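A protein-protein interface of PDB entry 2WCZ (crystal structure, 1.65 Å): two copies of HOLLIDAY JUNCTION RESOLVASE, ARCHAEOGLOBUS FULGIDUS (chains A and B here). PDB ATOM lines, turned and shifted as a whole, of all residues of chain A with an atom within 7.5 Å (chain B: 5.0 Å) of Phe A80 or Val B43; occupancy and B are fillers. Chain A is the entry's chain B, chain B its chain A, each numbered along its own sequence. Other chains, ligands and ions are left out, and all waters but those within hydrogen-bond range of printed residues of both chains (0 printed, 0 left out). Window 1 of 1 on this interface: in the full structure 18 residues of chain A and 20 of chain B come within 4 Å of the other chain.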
ATOM      1  N   ALA A  26     -10.597  -9.687   8.673  1.00  0.00           N
ATOM      2  CA  ALA A  26      -9.212  -9.926   8.289  1.00  0.00           C
ATOM      3  C   ALA A  26      -8.302  -8.885   8.909  1.00  0.00           C
ATOM      4  O   ALA A  26      -8.687  -7.733   9.086  1.00  0.00           O
ATOM      5  CB  ALA A  26      -9.076  -9.899   6.777  1.00  0.00           C
ATOM      6  N   ILE A  27      -7.099  -9.305   9.261  1.00  0.00           N
ATOM      7  CA  ILE A  27      -6.098  -8.393   9.789  1.00  0.00           C
ATOM      8  C   ILE A  27      -4.765  -8.588   9.068  1.00  0.00           C
ATOM      9  O   ILE A  27      -4.459  -9.685   8.600  1.00  0.00           O
ATOM     10  CB  ILE A  27      -5.880  -8.589  11.307  1.00  0.00           C
ATOM     11  CG1 ILE A  27      -5.549 -10.048  11.633  1.00  0.00           C
ATOM     12  CG2 ILE A  27      -7.113  -8.122  12.079  1.00  0.00           C
ATOM     13  CD1 ILE A  27      -4.080 -10.406  11.451  1.00  0.00           C
ATOM     14  N   PRO A  40       2.127 -15.369   8.740  1.00  0.00           N
ATOM     15  CA  PRO A  40       1.705 -14.995   7.391  1.00  0.00           C
ATOM     16  C   PRO A  40       1.619 -13.475   7.260  1.00  0.00           C
ATOM     17  O   PRO A  40       1.983 -12.770   8.194  1.00  0.00           O
ATOM     18  CB  PRO A  40       0.305 -15.621   7.269  1.00  0.00           C
ATOM     19  CG  PRO A  40      -0.114 -16.010   8.682  1.00  0.00           C
ATOM     20  CD  PRO A  40       0.973 -15.594   9.626  1.00  0.00           C
ATOM     21  N   VAL A  43      -4.261 -12.708   8.232  1.00  0.00           N
ATOM     22  CA  VAL A  43      -5.041 -13.800   8.786  1.00  0.00           C
ATOM     23  C   VAL A  43      -6.494 -13.360   8.690  1.00  0.00           C
ATOM     24  O   VAL A  43      -6.802 -12.199   8.929  1.00  0.00           O
ATOM     25  CB  VAL A  43      -4.652 -14.064  10.254  1.00  0.00           C
ATOM     26  CG1 VAL A  43      -5.556 -15.106  10.876  1.00  0.00           C
ATOM     27  CG2 VAL A  43      -3.193 -14.509  10.346  1.00  0.00           C
ATOM     28  N   ALA A  44      -7.380 -14.274   8.322  1.00  0.00           N
ATOM     29  CA  ALA A  44      -8.778 -13.937   8.133  1.00  0.00           C
ATOM     30  C   ALA A  44      -9.660 -15.062   8.654  1.00  0.00           C
ATOM     31  O   ALA A  44      -9.247 -16.226   8.701  1.00  0.00           O
ATOM     32  CB  ALA A  44      -9.059 -13.702   6.657  1.00  0.00           C
ATOM     33  N   GLY A  45     -10.877 -14.715   9.047  1.00  0.00           N
ATOM     34  CA  GLY A  45     -11.840 -15.727   9.434  1.00  0.00           C
ATOM     35  C   GLY A  45     -13.257 -15.253   9.209  1.00  0.00           C
ATOM     36  O   GLY A  45     -13.534 -14.057   9.229  1.00  0.00           O
ATOM     37  N   TYR A  50     -10.991 -20.301   8.262  1.00  0.00           N
ATOM     38  CA  TYR A  50      -9.908 -19.414   8.677  1.00  0.00           C
ATOM     39  C   TYR A  50      -8.809 -19.526   7.633  1.00  0.00           C
ATOM     40  O   TYR A  50      -8.551 -20.616   7.106  1.00  0.00           O
ATOM     41  CB  TYR A  50      -9.388 -19.823  10.054  1.00  0.00           C
ATOM     42  CG  TYR A  50     -10.453 -19.765  11.132  1.00  0.00           C
ATOM     43  CD1 TYR A  50     -10.723 -18.584  11.805  1.00  0.00           C
ATOM     44  CD2 TYR A  50     -11.207 -20.886  11.457  1.00  0.00           C
ATOM     45  CE1 TYR A  50     -11.704 -18.516  12.792  1.00  0.00           C
ATOM     46  CE2 TYR A  50     -12.190 -20.831  12.441  1.00  0.00           C
ATOM     47  CZ  TYR A  50     -12.438 -19.651  13.101  1.00  0.00           C
ATOM     48  OH  TYR A  50     -13.420 -19.620  14.074  1.00  0.00           O
ATOM     49  N   LEU A  51      -8.174 -18.397   7.344  1.00  0.00           N
ATOM     50  CA  LEU A  51      -7.182 -18.295   6.276  1.00  0.00           C
ATOM     51  C   LEU A  51      -5.889 -17.716   6.822  1.00  0.00           C
ATOM     52  O   LEU A  51      -5.898 -16.758   7.592  1.00  0.00           O
ATOM     53  CB  LEU A  51      -7.689 -17.364   5.173  1.00  0.00           C
ATOM     54  CG  LEU A  51      -9.077 -17.613   4.577  1.00  0.00           C
ATOM     55  CD1 LEU A  51      -9.402 -16.560   3.524  1.00  0.00           C
ATOM     56  CD2 LEU A  51      -9.160 -19.002   3.967  1.00  0.00           C
ATOM     57  N   ALA A  52      -4.771 -18.301   6.412  1.00  0.00           N
ATOM     58  CA  ALA A  52      -3.465 -17.738   6.690  1.00  0.00           C
ATOM     59  C   ALA A  52      -2.866 -17.503   5.318  1.00  0.00           C
ATOM     60  O   ALA A  52      -2.697 -18.441   4.545  1.00  0.00           O
ATOM     61  CB  ALA A  52      -2.617 -18.707   7.500  1.00  0.00           C
ATOM     62  N   VAL A  74       2.728 -22.932   6.118  1.00  0.00           N
ATOM     63  CA  VAL A  74       2.015 -24.172   6.401  1.00  0.00           C
ATOM     64  C   VAL A  74       2.070 -24.517   7.890  1.00  0.00           C
ATOM     65  O   VAL A  74       1.081 -24.992   8.461  1.00  0.00           O
ATOM     66  CB  VAL A  74       2.585 -25.352   5.568  1.00  0.00           C
ATOM     67  CG1 VAL A  74       2.081 -26.686   6.125  1.00  0.00           C
ATOM     68  CG2 VAL A  74       2.212 -25.186   4.093  1.00  0.00           C
ATOM     69  N   THR A  75       3.221 -24.265   8.515  1.00  0.00           N
ATOM     70  CA  THR A  75       3.396 -24.528   9.942  1.00  0.00           C
ATOM     71  C   THR A  75       2.493 -23.613  10.759  1.00  0.00           C
ATOM     72  O   THR A  75       1.854 -24.057  11.702  1.00  0.00           O
ATOM     73  CB  THR A  75       4.857 -24.326  10.397  1.00  0.00           C
ATOM     74  OG1 THR A  75       5.695 -25.304   9.766  1.00  0.00           O
ATOM     75  CG2 THR A  75       4.972 -24.467  11.922  1.00  0.00           C
ATOM     76  N   PHE A  76       2.435 -22.340  10.390  1.00  0.00           N
ATOM     77  CA  PHE A  76       1.544 -21.409  11.086  1.00  0.00           C
ATOM     78  C   PHE A  76       0.107 -21.859  10.908  1.00  0.00           C
ATOM     79  O   PHE A  76      -0.660 -21.907  11.863  1.00  0.00           O
ATOM     80  CB  PHE A  76       1.673 -19.988  10.542  1.00  0.00           C
ATOM     81  CG  PHE A  76       0.729 -19.028  11.198  1.00  0.00           C
ATOM     82  CD1 PHE A  76       1.092 -18.368  12.363  1.00  0.00           C
ATOM     83  CD2 PHE A  76      -0.539 -18.830  10.680  1.00  0.00           C
ATOM     84  CE1 PHE A  76       0.209 -17.499  12.987  1.00  0.00           C
ATOM     85  CE2 PHE A  76      -1.429 -17.967  11.297  1.00  0.00           C
ATOM     86  CZ  PHE A  76      -1.054 -17.305  12.452  1.00  0.00           C
ATOM     87  N   ALA A  77      -0.256 -22.190   9.674  1.00  0.00           N
ATOM     88  CA  ALA A  77      -1.632 -22.575   9.379  1.00  0.00           C
ATOM     89  C   ALA A  77      -2.032 -23.807  10.180  1.00  0.00           C
ATOM     90  O   ALA A  77      -3.132 -23.877  10.723  1.00  0.00           O
ATOM     91  CB  ALA A  77      -1.798 -22.829   7.885  1.00  0.00           C
ATOM     92  N   ARG A  78      -1.136 -24.783  10.262  1.00  0.00           N
ATOM     93  CA  ARG A  78      -1.418 -25.995  11.028  1.00  0.00           C
ATOM     94  C   ARG A  78      -1.594 -25.669  12.520  1.00  0.00           C
ATOM     95  O   ARG A  78      -2.499 -26.186  13.187  1.00  0.00           O
ATOM     96  CB  ARG A  78      -0.296 -27.024  10.841  1.00  0.00           C
ATOM     97  CG  ARG A  78      -0.593 -28.356  11.517  1.00  0.00           C
ATOM     98  CD  ARG A  78       0.466 -29.414  11.222  1.00  0.00           C
ATOM     99  NE  ARG A  78       1.798 -29.008  11.663  1.00  0.00           N
ATOM    100  CZ  ARG A  78       2.799 -28.685  10.848  1.00  0.00           C
ATOM    101  NH1 ARG A  78       2.638 -28.723   9.530  1.00  0.00           N
ATOM    102  NH2 ARG A  78       3.971 -28.326  11.354  1.00  0.00           N
ATOM    103  N   GLY A  79      -0.737 -24.797  13.042  1.00  0.00           N
ATOM    104  CA  GLY A  79      -0.772 -24.453  14.458  1.00  0.00           C
ATOM    105  C   GLY A  79      -2.001 -23.640  14.821  1.00  0.00           C
ATOM    106  O   GLY A  79      -2.632 -23.864  15.854  1.00  0.00           O
ATOM    107  N   PHE A  80      -2.344 -22.705  13.941  1.00  0.00           N
ATOM    108  CA  PHE A  80      -3.443 -21.767  14.178  1.00  0.00           C
ATOM    109  C   PHE A  80      -4.802 -22.434  14.005  1.00  0.00           C
ATOM    110  O   PHE A  80      -5.761 -22.116  14.722  1.00  0.00           O
ATOM    111  CB  PHE A  80      -3.340 -20.611  13.181  1.00  0.00           C
ATOM    112  CG  PHE A  80      -4.290 -19.480  13.461  1.00  0.00           C
ATOM    113  CD1 PHE A  80      -3.899 -18.427  14.270  1.00  0.00           C
ATOM    114  CD2 PHE A  80      -5.563 -19.463  12.902  1.00  0.00           C
ATOM    115  CE1 PHE A  80      -4.769 -17.365  14.542  1.00  0.00           C
ATOM    116  CE2 PHE A  80      -6.443 -18.410  13.168  1.00  0.00           C
ATOM    117  CZ  PHE A  80      -6.041 -17.361  13.986  1.00  0.00           C
ATOM    118  N   GLY A  81      -4.878 -23.354  13.047  1.00  0.00           N
ATOM    119  CA  GLY A  81      -6.140 -23.901  12.592  1.00  0.00           C
ATOM    120  C   GLY A  81      -6.704 -23.073  11.444  1.00  0.00           C
ATOM    121  O   GLY A  81      -7.823 -22.548  11.518  1.00  0.00           O
ATOM    122  N   ALA A  82      -5.918 -22.936  10.385  1.00  0.00           N
ATOM    123  CA  ALA A  82      -6.327 -22.173   9.216  1.00  0.00           C
ATOM    124  C   ALA A  82      -5.890 -22.901   7.950  1.00  0.00           C
ATOM    125  O   ALA A  82      -5.067 -23.816   7.994  1.00  0.00           O
ATOM    126  CB  ALA A  82      -5.712 -20.767   9.245  1.00  0.00           C
ATOM    127  N   GLU A  83      -6.436 -22.476   6.821  1.00  0.00           N
ATOM    128  CA  GLU A  83      -6.009 -22.987   5.525  1.00  0.00           C
ATOM    129  C   GLU A  83      -4.938 -22.058   4.972  1.00  0.00           C
ATOM    130  O   GLU A  83      -5.104 -20.841   4.993  1.00  0.00           O
ATOM    131  CB  GLU A  83      -7.206 -23.050   4.581  1.00  0.00           C
ATOM    132  CG  GLU A  83      -8.380 -23.839   5.160  1.00  0.00           C
ATOM    133  CD  GLU A  83      -9.591 -23.858   4.251  1.00  0.00           C
ATOM    134  OE1 GLU A  83      -9.408 -23.913   3.018  1.00  0.00           O
ATOM    135  OE2 GLU A  83     -10.729 -23.831   4.770  1.00  0.00           O
ATOM    136  N   ALA B  25      -0.755 -20.536  18.005  1.00  0.00           N
ATOM    137  CA  ALA B  25      -0.114 -19.715  16.989  1.00  0.00           C
ATOM    138  C   ALA B  25      -0.763 -18.337  17.110  1.00  0.00           C
ATOM    139  O   ALA B  25      -1.989 -18.227  17.095  1.00  0.00           O
ATOM    140  CB  ALA B  25      -0.341 -20.298  15.611  1.00  0.00           C
ATOM    141  N   ALA B  26       0.042 -17.286  17.246  1.00  0.00           N
ATOM    142  CA  ALA B  26      -0.503 -15.954  17.527  1.00  0.00           C
ATOM    143  C   ALA B  26       0.242 -14.902  16.713  1.00  0.00           C
ATOM    144  O   ALA B  26       1.434 -15.058  16.418  1.00  0.00           O
ATOM    145  CB  ALA B  26      -0.401 -15.643  19.021  1.00  0.00           C
ATOM    146  N   ILE B  27      -0.473 -13.850  16.332  1.00  0.00           N
ATOM    147  CA  ILE B  27       0.118 -12.731  15.609  1.00  0.00           C
ATOM    148  C   ILE B  27      -0.325 -11.417  16.230  1.00  0.00           C
ATOM    149  O   ILE B  27      -1.419 -11.329  16.783  1.00  0.00           O
ATOM    150  CB  ILE B  27      -0.264 -12.717  14.102  1.00  0.00           C
ATOM    151  CG1 ILE B  27      -1.784 -12.768  13.916  1.00  0.00           C
ATOM    152  CG2 ILE B  27       0.415 -13.868  13.372  1.00  0.00           C
ATOM    153  CD1 ILE B  27      -2.414 -11.417  13.752  1.00  0.00           C
ATOM    154  N   VAL B  29      -1.509  -7.583  15.511  1.00  0.00           N
ATOM    155  CA  VAL B  29      -2.264  -6.944  14.446  1.00  0.00           C
ATOM    156  C   VAL B  29      -1.612  -5.642  14.059  1.00  0.00           C
ATOM    157  O   VAL B  29      -1.394  -4.764  14.894  1.00  0.00           O
ATOM    158  CB  VAL B  29      -3.731  -6.704  14.880  1.00  0.00           C
ATOM    159  CG1 VAL B  29      -4.491  -5.892  13.834  1.00  0.00           C
ATOM    160  CG2 VAL B  29      -4.411  -8.023  15.133  1.00  0.00           C
ATOM    161  N   PRO B  40      -8.467  -6.284  16.914  1.00  0.00           N
ATOM    162  CA  PRO B  40      -7.871  -6.449  18.238  1.00  0.00           C
ATOM    163  C   PRO B  40      -6.371  -6.184  18.176  1.00  0.00           C
ATOM    164  O   PRO B  40      -5.855  -5.733  17.150  1.00  0.00           O
ATOM    165  CB  PRO B  40      -8.164  -7.918  18.541  1.00  0.00           C
ATOM    166  CG  PRO B  40      -7.955  -8.572  17.218  1.00  0.00           C
ATOM    167  CD  PRO B  40      -8.510  -7.574  16.194  1.00  0.00           C
ATOM    168  N   ASP B  41      -5.666  -6.447  19.270  1.00  0.00           N
ATOM    169  CA  ASP B  41      -4.221  -6.257  19.292  1.00  0.00           C
ATOM    170  C   ASP B  41      -3.506  -7.528  18.870  1.00  0.00           C
ATOM    171  O   ASP B  41      -2.490  -7.476  18.184  1.00  0.00           O
ATOM    172  CB  ASP B  41      -3.759  -5.841  20.692  1.00  0.00           C
ATOM    173  CG  ASP B  41      -4.272  -4.466  21.083  1.00  0.00           C
ATOM    174  OD1 ASP B  41      -4.370  -3.598  20.200  1.00  0.00           O
ATOM    175  OD2 ASP B  41      -4.595  -4.248  22.260  1.00  0.00           O
ATOM    176  N   ILE B  42      -4.053  -8.666  19.285  1.00  0.00           N
ATOM    177  CA  ILE B  42      -3.481  -9.973  18.964  1.00  0.00           C
ATOM    178  C   ILE B  42      -4.610 -10.904  18.529  1.00  0.00           C
ATOM    179  O   ILE B  42      -5.713 -10.856  19.060  1.00  0.00           O
ATOM    180  CB  ILE B  42      -2.751 -10.568  20.199  1.00  0.00           C
ATOM    181  CG1 ILE B  42      -1.408  -9.844  20.426  1.00  0.00           C
ATOM    182  CG2 ILE B  42      -2.568 -12.087  20.052  1.00  0.00           C
ATOM    183  CD1 ILE B  42      -0.691 -10.248  21.710  1.00  0.00           C
ATOM    184  N   VAL B  43      -4.336 -11.747  17.545  1.00  0.00           N
ATOM    185  CA  VAL B  43      -5.251 -12.819  17.200  1.00  0.00           C
ATOM    186  C   VAL B  43      -4.475 -14.123  17.358  1.00  0.00           C
ATOM    187  O   VAL B  43      -3.303 -14.209  16.977  1.00  0.00           O
ATOM    188  CB  VAL B  43      -5.784 -12.663  15.750  1.00  0.00           C
ATOM    189  CG1 VAL B  43      -6.638 -13.862  15.359  1.00  0.00           C
ATOM    190  CG2 VAL B  43      -6.589 -11.352  15.615  1.00  0.00           C
ATOM    191  N   ALA B  44      -5.118 -15.131  17.934  1.00  0.00           N
ATOM    192  CA  ALA B  44      -4.452 -16.391  18.204  1.00  0.00           C
ATOM    193  C   ALA B  44      -5.387 -17.568  17.948  1.00  0.00           C
ATOM    194  O   ALA B  44      -6.598 -17.419  17.993  1.00  0.00           O
ATOM    195  CB  ALA B  44      -3.969 -16.405  19.628  1.00  0.00           C
ATOM    196  N   GLY B  45      -4.818 -18.737  17.683  1.00  0.00           N
ATOM    197  CA  GLY B  45      -5.613 -19.935  17.480  1.00  0.00           C
ATOM    198  C   GLY B  45      -4.770 -21.172  17.750  1.00  0.00           C
ATOM    199  O   GLY B  45      -3.548 -21.139  17.582  1.00  0.00           O
ATOM    200  N   ASN B  46      -5.409 -22.248  18.203  1.00  0.00           N
ATOM    201  CA  ASN B  46      -4.702 -23.514  18.410  1.00  0.00           C
ATOM    202  C   ASN B  46      -5.422 -24.674  17.716  1.00  0.00           C
ATOM    203  O   ASN B  46      -5.185 -25.840  18.031  1.00  0.00           O
ATOM    204  CB  ASN B  46      -4.532 -23.799  19.902  1.00  0.00           C
ATOM    205  CG  ASN B  46      -5.853 -24.064  20.585  1.00  0.00           C
ATOM    206  OD1 ASN B  46      -6.884 -24.149  19.921  1.00  0.00           O
ATOM    207  ND2 ASN B  46      -5.837 -24.199  21.908  1.00  0.00           N
ATOM    208  N   GLY B  47      -6.300 -24.345  16.770  1.00  0.00           N
ATOM    209  CA  GLY B  47      -7.020 -25.349  16.002  1.00  0.00           C
ATOM    210  C   GLY B  47      -8.420 -25.594  16.526  1.00  0.00           C
ATOM    211  O   GLY B  47      -9.284 -26.098  15.808  1.00  0.00           O
ATOM    212  N   TYR B  50     -10.104 -20.010  19.245  1.00  0.00           N
ATOM    213  CA  TYR B  50      -9.566 -18.840  18.552  1.00  0.00           C
ATOM    214  C   TYR B  50      -9.801 -17.626  19.437  1.00  0.00           C
ATOM    215  O   TYR B  50     -10.863 -17.514  20.060  1.00  0.00           O
ATOM    216  CB  TYR B  50     -10.245 -18.643  17.191  1.00  0.00           C
ATOM    217  CG  TYR B  50     -10.017 -19.792  16.239  1.00  0.00           C
ATOM    218  CD1 TYR B  50      -8.930 -19.792  15.372  1.00  0.00           C
ATOM    219  CD2 TYR B  50     -10.874 -20.878  16.224  1.00  0.00           C
ATOM    220  CE1 TYR B  50      -8.703 -20.854  14.497  1.00  0.00           C
ATOM    221  CE2 TYR B  50     -10.665 -21.945  15.348  1.00  0.00           C
ATOM    222  CZ  TYR B  50      -9.573 -21.921  14.493  1.00  0.00           C
ATOM    223  OH  TYR B  50      -9.359 -22.972  13.624  1.00  0.00           O
ATOM    224  N   LEU B  51      -8.817 -16.733  19.517  1.00  0.00           N
ATOM    225  CA  LEU B  51      -8.866 -15.615  20.451  1.00  0.00           C
ATOM    226  C   LEU B  51      -8.683 -14.294  19.730  1.00  0.00           C
ATOM    227  O   LEU B  51      -7.851 -14.186  18.822  1.00  0.00           O
ATOM    228  CB  LEU B  51      -7.763 -15.743  21.507  1.00  0.00           C
ATOM    229  CG  LEU B  51      -7.701 -17.064  22.275  1.00  0.00           C
ATOM    230  CD1 LEU B  51      -6.502 -17.048  23.234  1.00  0.00           C
ATOM    231  CD2 LEU B  51      -8.993 -17.335  23.038  1.00  0.00           C
ATOM    232  N   ALA B  52      -9.469 -13.299  20.140  1.00  0.00           N
ATOM    233  CA  ALA B  52      -9.280 -11.905  19.731  1.00  0.00           C
ATOM    234  C   ALA B  52      -8.994 -11.154  21.014  1.00  0.00           C
ATOM    235  O   ALA B  52      -9.833 -11.124  21.912  1.00  0.00           O
ATOM    236  CB  ALA B  52     -10.532 -11.360  19.068  1.00  0.00           C
ATOM    237  N   PHE B  76     -15.438  -7.554  16.137  1.00  0.00           N
ATOM    238  CA  PHE B  76     -14.404  -8.287  15.397  1.00  0.00           C
ATOM    239  C   PHE B  76     -14.469  -9.776  15.717  1.00  0.00           C
ATOM    240  O   PHE B  76     -14.434 -10.611  14.820  1.00  0.00           O
ATOM    241  CB  PHE B  76     -12.994  -7.790  15.709  1.00  0.00           C
ATOM    242  CG  PHE B  76     -11.921  -8.636  15.078  1.00  0.00           C
ATOM    243  CD1 PHE B  76     -11.473  -8.371  13.788  1.00  0.00           C
ATOM    244  CD2 PHE B  76     -11.391  -9.730  15.760  1.00  0.00           C
ATOM    245  CE1 PHE B  76     -10.498  -9.165  13.199  1.00  0.00           C
ATOM    246  CE2 PHE B  76     -10.423 -10.536  15.171  1.00  0.00           C
ATOM    247  CZ  PHE B  76      -9.977 -10.254  13.884  1.00  0.00           C
ATOM    248  N   PHE B  80     -14.996 -12.708  12.968  1.00  0.00           N
ATOM    249  CA  PHE B  80     -13.875 -13.606  12.721  1.00  0.00           C
ATOM    250  C   PHE B  80     -14.188 -15.036  13.130  1.00  0.00           C
ATOM    251  O   PHE B  80     -13.740 -15.980  12.481  1.00  0.00           O
ATOM    252  CB  PHE B  80     -12.651 -13.121  13.514  1.00  0.00           C
ATOM    253  CG  PHE B  80     -11.373 -13.862  13.201  1.00  0.00           C
ATOM    254  CD1 PHE B  80     -10.509 -13.378  12.228  1.00  0.00           C
ATOM    255  CD2 PHE B  80     -11.007 -15.005  13.913  1.00  0.00           C
ATOM    256  CE1 PHE B  80      -9.303 -14.026  11.935  1.00  0.00           C
ATOM    257  CE2 PHE B  80      -9.795 -15.672  13.617  1.00  0.00           C
ATOM    258  CZ  PHE B  80      -8.951 -15.178  12.640  1.00  0.00           C
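O of Phe A80 is in hydrogen-bond range of N of Gly B47 (3.1 Å).
The side-chain hydroxyl (OH) of Tyr B50 is in hydrogen-bond range of the backbone carbonyl oxygen (O) of Gly A81 (2.6 Å).
The backbone carbonyl oxygen of Gly A79 lies close to the backbone carbonyl oxygen of Gly B45 (3.4 Å).
N of Ala B25 sits at hydrogen-bond distance from O of Gly B45, 2.9 Å away.
The backbone NH (N) of Ile B27 sits at hydrogen-bond distance from the backbone carbonyl oxygen (O) of Val B43 (2.9 Å).
The backbone NH (N) of Val B29 sits at hydrogen-bond distance from the backbone carbonyl oxygen (O) of Asp B41, 2.8 Å away.
N of Leu B51 is in hydrogen-bond range of O of Ala B44, at 2.8 Å.
O of Ala A44 lies within hydrogen-bond range of N of Leu A51 (2.8 Å).
O of Tyr A50 sits at hydrogen-bond distance from N of Glu A83, 2.8 Å away.
Among the printed residues, merely in contact across the chains: Ile A27 with Ile B27, Ile A27 with Val B29, Ile A27 with Phe B76, Val A43 with Phe B80, Ala A44 with Phe B80, Gly A45 with Phe B80, Tyr A50 with Tyr B50, Tyr A50 with Phe B80, Phe A76 with Ala B25, Phe A76 with Ile B27, Gly A79 with Ala B25, Gly A79 with Asn B46, Gly A79 with Gly B47, Phe A80 with Ala B25, Phe A80 with Val B43, Phe A80 with Ala B44, Phe A80 with Gly B45, Phe A80 with Asn B46, Phe A80 with Tyr B50, Phe A80 with Phe B80 and Gly A81 with Gly B47.
Printed residues of chain B within 4 Å of Phe A76: Ala B25 and Ile B27.
Of chain B, only Ala B25, Val B43, Ala B44, Gly B45, Asn B46, Gly B47, Tyr B50 and Phe B80 come within 4 Å of Phe A80.
Val B43 touches just one residue of chain A: Phe A80.
Of the printed residues of chain A, Gly B47 touches Gly A79 (3.8 Å), Phe A80 (3.1 Å) and Gly A81 (3.8 Å).
The nearest residue of chain A that does not touch Val B43 is Ile A27 (4.3 Å).
Of the 17 printed residues of chain B, 11 touch a printed residue of chain A.
Hydrophobic or aromatic side chains of chain B that line the printed part of chain A: Ala B25, Ile B27, Val B29, Val B43, Tyr B50, Phe B76 and Phe B80.
Of the 19 printed residues of chain A, 9 touch a printed residue of chain B.
Printed residues of chain A that touch a printed residue of chain B: Ile A27, Val A43, Ala A44, Gly A45, Tyr A50, Phe A76, Gly A79, Phe A80 and Gly A81.
Along chain A the printed residues that touch a printed residue of chain B span positions 27 to 81.
Among the printed residues, 24 pairs touch across the chains.
Ile A27 touches Phe B76, and with the chains exchanged Phe A76 touches Ile B27.
Gly A45 touches Phe B80, and with the chains exchanged Phe A80 touches Gly B45.
Tyr A50 touches its own counterpart, Tyr B50.
Phe B80 touches its own counterpart, Phe A80.
Positions printed for both chains: 26, 27, 40, 43, 44, 45, 50, 51, 52, 76 and 80.
Of the 24 pairs that touch across the chains among the printed residues, 13 have their exchanged pair printed and touching as well.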
